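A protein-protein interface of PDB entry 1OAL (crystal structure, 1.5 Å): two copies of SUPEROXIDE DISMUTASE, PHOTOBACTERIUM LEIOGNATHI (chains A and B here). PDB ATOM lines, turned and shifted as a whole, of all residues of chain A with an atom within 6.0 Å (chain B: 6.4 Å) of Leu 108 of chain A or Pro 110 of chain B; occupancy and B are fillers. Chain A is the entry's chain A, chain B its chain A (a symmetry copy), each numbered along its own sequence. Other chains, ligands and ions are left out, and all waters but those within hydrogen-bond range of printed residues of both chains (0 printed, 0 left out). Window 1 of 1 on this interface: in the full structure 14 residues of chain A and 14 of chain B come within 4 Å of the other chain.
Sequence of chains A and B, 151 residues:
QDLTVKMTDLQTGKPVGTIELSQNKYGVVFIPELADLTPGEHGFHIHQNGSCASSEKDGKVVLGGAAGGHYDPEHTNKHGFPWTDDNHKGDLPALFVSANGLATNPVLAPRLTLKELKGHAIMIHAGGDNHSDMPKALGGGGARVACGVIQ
Tyr 26 of chain A touches Pro 110 of chain B, and with the chains exchanged Pro 110 of chain A touches Tyr 26 of chain B.
Leu 108 of chain A touches Pro 110 of chain B, and with the chains exchanged Pro 110 of chain A touches Leu 108 of chain B.
Of the 12 printed residues of chain B, 5 touch a printed residue of chain A.
Hydrophobic or aromatic side chains of chain B within 4 Å of the printed part of chain A: Tyr 26, Trp 83, Leu 108 and Pro 110.
Of the 14 printed residues of chain A, 6 touch a printed residue of chain B.
Printed residues of chain A that touch a printed residue of chain B: Asn 24, Tyr 26, Val 29, Pro 106, Leu 108 and Pro 110.
Along chain A the printed residues that touch a printed residue of chain B span positions 24 to 110.
Among the printed residues, 10 pairs touch across the chains.
Among the printed residues, no Asp or Glu carboxylate lies within 4 Å of a Lys or Arg side-chain nitrogen of the other chain.
Among the printed residues, merely in contact across the chains: Tyr 26 of chain A with Arg 111 of chain B (3.4 Å), Tyr 26 of chain A with Trp 83 of chain B (3.4 Å), Asn 24 of chain A with Trp 83 of chain B (3.4 Å), Val 29 of chain A with Trp 83 of chain B (3.6 Å), Pro 106 of chain A with Trp 83 of chain B (3.7 Å), Leu 108 of chain A with Trp 83 of chain B (3.7 Å), Leu 108 of chain A with Pro 110 of chain B (3.7 Å), Pro 110 of chain A with Leu 108 of chain B (3.7 Å), Tyr 26 of chain A with Pro 110 of chain B (3.8 Å) and Pro 110 of chain A with Tyr 26 of chain B (3.8 Å).
Leu 108 of chain A touches just these residues of chain B: Trp 83 (3.7 Å) and Pro 110 (3.7 Å).
Of chain A, only Tyr 26 and Leu 108 come within 4 Å of Pro 110 of chain B.
Printed residues of chain B within 4 Å of Tyr 26 of chain A: Trp 83 (3.4 Å), Pro 110 (3.8 Å) and Arg 111 (3.4 Å).
Printed residues of chain A within 4 Å of Arg 111 of chain B: Tyr 26 (3.4 Å).
Of the printed residues of chain B, Asn 24 of chain A touches Trp 83.
Val 107 of chain A touches none of the printed residues of chain B.
The nearest printed residue of chain A that does not touch Pro 110 of chain B is Pro 110 of chain A (6.0 Å).
The side-chain amide oxygen of Asn 24 of chain A lies within hydrogen-bond range of the backbone NH of Tyr 26 of chain A (2.8 Å).
O of Pro 82 of chain B sits at hydrogen-bond distance from NE of Arg 111 of chain B.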
ATOM      1  N   ASN A  24     -21.221  20.103  -5.606  1.00  0.00           N
ATOM      2  CA  ASN A  24     -19.753  20.106  -5.865  1.00  0.00           C
ATOM      3  C   ASN A  24     -18.959  20.523  -4.680  1.00  0.00           C
ATOM      4  O   ASN A  24     -19.525  20.766  -3.618  1.00  0.00           O
ATOM      5  CB  ASN A  24     -19.291  20.810  -7.159  1.00  0.00           C
ATOM      6  CG  ASN A  24     -19.485  22.334  -7.128  1.00  0.00           C
ATOM      7  OD1 ASN A  24     -18.849  23.055  -6.336  1.00  0.00           O
ATOM      8  ND2 ASN A  24     -20.304  22.826  -8.023  1.00  0.00           N
ATOM      9  N   TYR A  26     -17.650  23.082  -3.804  1.00  0.00           N
ATOM     10  CA  TYR A  26     -17.848  24.430  -3.295  1.00  0.00           C
ATOM     11  C   TYR A  26     -19.244  24.731  -2.785  1.00  0.00           C
ATOM     12  O   TYR A  26     -19.476  25.831  -2.274  1.00  0.00           O
ATOM     13  CB  TYR A  26     -17.457  25.463  -4.353  1.00  0.00           C
ATOM     14  CG  TYR A  26     -16.051  25.267  -4.841  1.00  0.00           C
ATOM     15  CD1 TYR A  26     -15.794  24.734  -6.095  1.00  0.00           C
ATOM     16  CD2 TYR A  26     -14.976  25.607  -4.039  1.00  0.00           C
ATOM     17  CE1 TYR A  26     -14.489  24.530  -6.523  1.00  0.00           C
ATOM     18  CE2 TYR A  26     -13.669  25.422  -4.484  1.00  0.00           C
ATOM     19  CZ  TYR A  26     -13.447  24.878  -5.722  1.00  0.00           C
ATOM     20  OH  TYR A  26     -12.147  24.673  -6.164  1.00  0.00           O
ATOM     21  N   GLY A  27     -20.160  23.775  -2.912  1.00  0.00           N
ATOM     22  CA  GLY A  27     -21.521  23.945  -2.441  1.00  0.00           C
ATOM     23  C   GLY A  27     -22.531  23.345  -3.392  1.00  0.00           C
ATOM     24  O   GLY A  27     -22.191  22.479  -4.190  1.00  0.00           O
ATOM     25  N   VAL A  28     -23.774  23.798  -3.308  1.00  0.00           N
ATOM     26  CA  VAL A  28     -24.816  23.312  -4.198  1.00  0.00           C
ATOM     27  C   VAL A  28     -25.020  24.288  -5.345  1.00  0.00           C
ATOM     28  O   VAL A  28     -25.171  25.474  -5.128  1.00  0.00           O
ATOM     29  CB  VAL A  28     -26.139  23.110  -3.446  1.00  0.00           C
ATOM     30  CG1 VAL A  28     -27.255  22.762  -4.412  1.00  0.00           C
ATOM     31  CG2 VAL A  28     -25.978  21.977  -2.422  1.00  0.00           C
ATOM     32  N   VAL A  29     -24.997  23.780  -6.561  1.00  0.00           N
ATOM     33  CA  VAL A  29     -25.247  24.623  -7.745  1.00  0.00           C
ATOM     34  C   VAL A  29     -26.685  24.391  -8.208  1.00  0.00           C
ATOM     35  O   VAL A  29     -27.172  23.248  -8.332  1.00  0.00           O
ATOM     36  CB  VAL A  29     -24.281  24.292  -8.891  1.00  0.00           C
ATOM     37  CG1 VAL A  29     -24.606  25.133 -10.137  1.00  0.00           C
ATOM     38  CG2 VAL A  29     -22.820  24.583  -8.448  1.00  0.00           C
ATOM     39  N   PHE A  30     -27.378  25.490  -8.425  1.00  0.00           N
ATOM     40  CA  PHE A  30     -28.750  25.476  -8.909  1.00  0.00           C
ATOM     41  C   PHE A  30     -28.720  25.930 -10.355  1.00  0.00           C
ATOM     42  O   PHE A  30     -28.339  27.052 -10.623  1.00  0.00           O
ATOM     43  CB  PHE A  30     -29.594  26.472  -8.097  1.00  0.00           C
ATOM     44  CG  PHE A  30     -29.713  26.107  -6.625  1.00  0.00           C
ATOM     45  CD1 PHE A  30     -28.662  26.358  -5.742  1.00  0.00           C
ATOM     46  CD2 PHE A  30     -30.878  25.531  -6.135  1.00  0.00           C
ATOM     47  CE1 PHE A  30     -28.768  26.028  -4.407  1.00  0.00           C
ATOM     48  CE2 PHE A  30     -30.980  25.176  -4.804  1.00  0.00           C
ATOM     49  CZ  PHE A  30     -29.924  25.440  -3.940  1.00  0.00           C
ATOM     50  N   PRO A  82     -25.600  34.610   0.712  1.00  0.00           N
ATOM     51  CA  PRO A  82     -25.287  33.175   0.618  1.00  0.00           C
ATOM     52  C   PRO A  82     -23.949  32.814   1.235  1.00  0.00           C
ATOM     53  O   PRO A  82     -23.711  31.632   1.508  1.00  0.00           O
ATOM     54  CB  PRO A  82     -25.236  32.920  -0.904  1.00  0.00           C
ATOM     55  CG  PRO A  82     -25.989  34.105  -1.525  1.00  0.00           C
ATOM     56  CD  PRO A  82     -25.661  35.267  -0.614  1.00  0.00           C
ATOM     57  N   LEU A  92     -30.177  32.140  -1.157  1.00  0.00           N
ATOM     58  CA  LEU A  92     -29.413  31.821  -2.371  1.00  0.00           C
ATOM     59  C   LEU A  92     -29.083  33.118  -3.110  1.00  0.00           C
ATOM     60  O   LEU A  92     -29.687  34.150  -2.843  1.00  0.00           O
ATOM     61  CB  LEU A  92     -30.251  30.921  -3.315  1.00  0.00           C
ATOM     62  CG  LEU A  92     -30.878  29.696  -2.638  1.00  0.00           C
ATOM     63  CD1 LEU A  92     -31.786  28.932  -3.650  1.00  0.00           C
ATOM     64  CD2 LEU A  92     -29.777  28.772  -2.084  1.00  0.00           C
ATOM     65  N   PRO A  93     -28.138  33.088  -4.022  1.00  0.00           N
ATOM     66  CA  PRO A  93     -27.973  34.245  -4.921  1.00  0.00           C
ATOM     67  C   PRO A  93     -29.270  34.506  -5.671  1.00  0.00           C
ATOM     68  O   PRO A  93     -30.057  33.569  -5.944  1.00  0.00           O
ATOM     69  CB  PRO A  93     -26.847  33.797  -5.882  1.00  0.00           C
ATOM     70  CG  PRO A  93     -26.068  32.728  -5.059  1.00  0.00           C
ATOM     71  CD  PRO A  93     -27.175  31.989  -4.327  1.00  0.00           C
ATOM     72  N   PRO A 106     -26.891  29.822 -13.813  1.00  0.00           N
ATOM     73  CA  PRO A 106     -26.737  28.973 -12.614  1.00  0.00           C
ATOM     74  C   PRO A 106     -26.128  29.772 -11.489  1.00  0.00           C
ATOM     75  O   PRO A 106     -25.425  30.751 -11.763  1.00  0.00           O
ATOM     76  CB  PRO A 106     -25.762  27.896 -13.064  1.00  0.00           C
ATOM     77  CG  PRO A 106     -24.880  28.606 -14.101  1.00  0.00           C
ATOM     78  CD  PRO A 106     -25.865  29.544 -14.847  1.00  0.00           C
ATOM     79  N   VAL A 107     -26.430  29.383 -10.246  1.00  0.00           N
ATOM     80  CA  VAL A 107     -25.879  30.055  -9.098  1.00  0.00           C
ATOM     81  C   VAL A 107     -25.416  29.022  -8.060  1.00  0.00           C
ATOM     82  O   VAL A 107     -25.897  27.862  -8.027  1.00  0.00           O
ATOM     83  CB  VAL A 107     -26.884  31.035  -8.447  1.00  0.00           C
ATOM     84  CG1 VAL A 107     -27.302  32.122  -9.443  1.00  0.00           C
ATOM     85  CG2 VAL A 107     -28.108  30.292  -7.891  1.00  0.00           C
ATOM     86  N   LEU A 108     -24.502  29.453  -7.202  1.00  0.00           N
ATOM     87  CA  LEU A 108     -23.900  28.579  -6.179  1.00  0.00           C
ATOM     88  C   LEU A 108     -24.328  28.987  -4.765  1.00  0.00           C
ATOM     89  O   LEU A 108     -24.319  30.168  -4.422  1.00  0.00           O
ATOM     90  CB  LEU A 108     -22.359  28.683  -6.258  1.00  0.00           C
ATOM     91  CG  LEU A 108     -21.563  27.921  -5.168  1.00  0.00           C
ATOM     92  CD1 LEU A 108     -21.648  26.444  -5.449  1.00  0.00           C
ATOM     93  CD2 LEU A 108     -20.100  28.391  -5.211  1.00  0.00           C
ATOM     94  N   ALA A 109     -24.669  27.993  -3.942  1.00  0.00           N
ATOM     95  CA  ALA A 109     -24.882  28.221  -2.508  1.00  0.00           C
ATOM     96  C   ALA A 109     -23.777  27.485  -1.735  1.00  0.00           C
ATOM     97  O   ALA A 109     -23.858  26.276  -1.529  1.00  0.00           O
ATOM     98  CB  ALA A 109     -26.238  27.675  -2.091  1.00  0.00           C
ATOM     99  N   PRO A 110     -22.741  28.194  -1.327  1.00  0.00           N
ATOM    100  CA  PRO A 110     -21.597  27.529  -0.676  1.00  0.00           C
ATOM    101  C   PRO A 110     -21.924  26.931   0.692  1.00  0.00           C
ATOM    102  O   PRO A 110     -21.200  26.052   1.164  1.00  0.00           O
ATOM    103  CB  PRO A 110     -20.572  28.665  -0.540  1.00  0.00           C
ATOM    104  CG  PRO A 110     -21.412  29.904  -0.437  1.00  0.00           C
ATOM    105  CD  PRO A 110     -22.535  29.647  -1.448  1.00  0.00           C
ATOM    106  N   TYR B  26     -15.705  31.666   2.268  1.00  0.00           N
ATOM    107  CA  TYR B  26     -16.152  30.937   1.092  1.00  0.00           C
ATOM    108  C   TYR B  26     -15.530  31.377  -0.219  1.00  0.00           C
ATOM    109  O   TYR B  26     -15.805  30.763  -1.254  1.00  0.00           O
ATOM    110  CB  TYR B  26     -17.676  30.989   0.978  1.00  0.00           C
ATOM    111  CG  TYR B  26     -18.353  30.487   2.219  1.00  0.00           C
ATOM    112  CD1 TYR B  26     -18.964  31.359   3.107  1.00  0.00           C
ATOM    113  CD2 TYR B  26     -18.372  29.135   2.511  1.00  0.00           C
ATOM    114  CE1 TYR B  26     -19.562  30.886   4.267  1.00  0.00           C
ATOM    115  CE2 TYR B  26     -18.994  28.663   3.664  1.00  0.00           C
ATOM    116  CZ  TYR B  26     -19.576  29.551   4.530  1.00  0.00           C
ATOM    117  OH  TYR B  26     -20.180  29.090   5.691  1.00  0.00           O
ATOM    118  N   GLY B  27     -14.702  32.417  -0.183  1.00  0.00           N
ATOM    119  CA  GLY B  27     -14.035  32.912  -1.371  1.00  0.00           C
ATOM    120  C   GLY B  27     -13.974  34.422  -1.403  1.00  0.00           C
ATOM    121  O   GLY B  27     -14.083  35.068  -0.366  1.00  0.00           O
ATOM    122  N   VAL B  28     -13.796  34.989  -2.588  1.00  0.00           N
ATOM    123  CA  VAL B  28     -13.755  36.435  -2.734  1.00  0.00           C
ATOM    124  C   VAL B  28     -15.107  36.950  -3.197  1.00  0.00           C
ATOM    125  O   VAL B  28     -15.667  36.446  -4.151  1.00  0.00           O
ATOM    126  CB  VAL B  28     -12.667  36.862  -3.729  1.00  0.00           C
ATOM    127  CG1 VAL B  28     -12.744  38.353  -3.997  1.00  0.00           C
ATOM    128  CG2 VAL B  28     -11.285  36.516  -3.157  1.00  0.00           C
ATOM    129  N   PRO B  82     -17.341  29.324 -12.166  1.00  0.00           N
ATOM    130  CA  PRO B  82     -16.589  29.739 -10.971  1.00  0.00           C
ATOM    131  C   PRO B  82     -16.373  28.611  -9.980  1.00  0.00           C
ATOM    132  O   PRO B  82     -15.505  28.733  -9.108  1.00  0.00           O
ATOM    133  CB  PRO B  82     -17.496  30.815 -10.334  1.00  0.00           C
ATOM    134  CG  PRO B  82     -18.437  31.253 -11.465  1.00  0.00           C
ATOM    135  CD  PRO B  82     -18.660  29.990 -12.268  1.00  0.00           C
ATOM    136  N   TRP B  83     -17.092  27.512 -10.143  1.00  0.00           N
ATOM    137  CA  TRP B  83     -17.039  26.394  -9.195  1.00  0.00           C
ATOM    138  C   TRP B  83     -16.526  25.102  -9.844  1.00  0.00           C
ATOM    139  O   TRP B  83     -16.701  24.034  -9.291  1.00  0.00           O
ATOM    140  CB  TRP B  83     -18.410  26.128  -8.606  1.00  0.00           C
ATOM    141  CG  TRP B  83     -19.506  26.142  -9.660  1.00  0.00           C
ATOM    142  CD1 TRP B  83     -19.849  25.128 -10.510  1.00  0.00           C
ATOM    143  CD2 TRP B  83     -20.366  27.234  -9.981  1.00  0.00           C
ATOM    144  NE1 TRP B  83     -20.880  25.517 -11.333  1.00  0.00           N
ATOM    145  CE2 TRP B  83     -21.234  26.799 -11.010  1.00  0.00           C
ATOM    146  CE3 TRP B  83     -20.529  28.531  -9.461  1.00  0.00           C
ATOM    147  CZ2 TRP B  83     -22.205  27.622 -11.577  1.00  0.00           C
ATOM    148  CZ3 TRP B  83     -21.524  29.358 -10.018  1.00  0.00           C
ATOM    149  CH2 TRP B  83     -22.345  28.898 -11.063  1.00  0.00           C
ATOM    150  N   PRO B  93     -18.803  34.680 -11.570  1.00  0.00           N
ATOM    151  CA  PRO B  93     -20.222  34.725 -11.969  1.00  0.00           C
ATOM    152  C   PRO B  93     -20.480  35.953 -12.827  1.00  0.00           C
ATOM    153  O   PRO B  93     -19.807  37.000 -12.673  1.00  0.00           O
ATOM    154  CB  PRO B  93     -20.972  34.812 -10.619  1.00  0.00           C
ATOM    155  CG  PRO B  93     -19.975  34.179  -9.604  1.00  0.00           C
ATOM    156  CD  PRO B  93     -18.628  34.688 -10.088  1.00  0.00           C
ATOM    157  N   LEU B 108     -19.877  35.859  -5.739  1.00  0.00           N
ATOM    158  CA  LEU B 108     -18.807  35.132  -5.033  1.00  0.00           C
ATOM    159  C   LEU B 108     -17.949  34.310  -6.001  1.00  0.00           C
ATOM    160  O   LEU B 108     -18.471  33.622  -6.876  1.00  0.00           O
ATOM    161  CB  LEU B 108     -19.438  34.156  -4.013  1.00  0.00           C
ATOM    162  CG  LEU B 108     -18.458  33.215  -3.264  1.00  0.00           C
ATOM    163  CD1 LEU B 108     -17.677  34.026  -2.264  1.00  0.00           C
ATOM    164  CD2 LEU B 108     -19.273  32.124  -2.551  1.00  0.00           C
ATOM    165  N   ALA B 109     -16.628  34.366  -5.811  1.00  0.00           N
ATOM    166  CA  ALA B 109     -15.711  33.464  -6.516  1.00  0.00           C
ATOM    167  C   ALA B 109     -15.070  32.525  -5.482  1.00  0.00           C
ATOM    168  O   ALA B 109     -14.125  32.907  -4.795  1.00  0.00           O
ATOM    169  CB  ALA B 109     -14.624  34.267  -7.211  1.00  0.00           C
ATOM    170  N   PRO B 110     -15.584  31.317  -5.352  1.00  0.00           N
ATOM    171  CA  PRO B 110     -15.086  30.408  -4.303  1.00  0.00           C
ATOM    172  C   PRO B 110     -13.647  29.940  -4.520  1.00  0.00           C
ATOM    173  O   PRO B 110     -12.996  29.502  -3.570  1.00  0.00           O
ATOM    174  CB  PRO B 110     -16.059  29.223  -4.385  1.00  0.00           C
ATOM    175  CG  PRO B 110     -16.505  29.215  -5.818  1.00  0.00           C
ATOM    176  CD  PRO B 110     -16.668  30.705  -6.139  1.00  0.00           C
ATOM    177  N   ARG B 111     -13.140  30.041  -5.745  1.00  0.00           N
ATOM    178  CA  ARG B 111     -11.808  29.509  -6.035  1.00  0.00           C
ATOM    179  C   ARG B 111     -10.676  30.529  -5.830  1.00  0.00           C
ATOM    180  O   ARG B 111      -9.497  30.171  -5.861  1.00  0.00           O
ATOM    181  CB  ARG B 111     -11.757  28.978  -7.482  1.00  0.00           C
ATOM    182  CG  ARG B 111     -12.508  27.678  -7.645  1.00  0.00           C
ATOM    183  CD  ARG B 111     -12.096  26.901  -8.901  1.00  0.00           C
ATOM    184  NE  ARG B 111     -12.622  27.626 -10.014  1.00  0.00           N
ATOM    185  CZ  ARG B 111     -12.001  27.902 -11.165  1.00  0.00           C
ATOM    186  NH1 ARG B 111     -10.748  27.492 -11.451  1.00  0.00           N
ATOM    187  NH2 ARG B 111     -12.678  28.621 -12.037  1.00  0.00           N
ATOM    188  N   LEU B 112     -11.025  31.790  -5.630  1.00  0.00           N
ATOM    189  CA  LEU B 112     -10.025  32.844  -5.545  1.00  0.00           C
ATOM    190  C   LEU B 112      -9.699  33.257  -4.118  1.00  0.00           C
ATOM    191  O   LEU B 112     -10.527  33.130  -3.207  1.00  0.00           O
ATOM    192  CB  LEU B 112     -10.505  34.079  -6.309  1.00  0.00           C
ATOM    193  CG  LEU B 112     -10.429  33.904  -7.847  1.00  0.00           C
ATOM    194  CD1 LEU B 112     -11.114  35.092  -8.506  1.00  0.00           C
ATOM    195  CD2 LEU B 112      -8.979  33.817  -8.336  1.00  0.00           C
ATOM    196  N   THR B 113      -8.481  33.736  -3.931  1.00  0.00           N
ATOM    197  CA  THR B 113      -8.135  34.437  -2.685  1.00  0.00           C
ATOM    198  C   THR B 113      -7.893  35.899  -3.021  1.00  0.00           C
ATOM    199  O   THR B 113      -7.510  36.245  -4.137  1.00  0.00           O
ATOM    200  CB  THR B 113      -6.874  33.859  -2.034  1.00  0.00           C
ATOM    201  OG1 THR B 113      -5.745  34.193  -2.856  1.00  0.00           O
ATOM    202  CG2 THR B 113      -6.933  32.339  -1.969  1.00  0.00           C
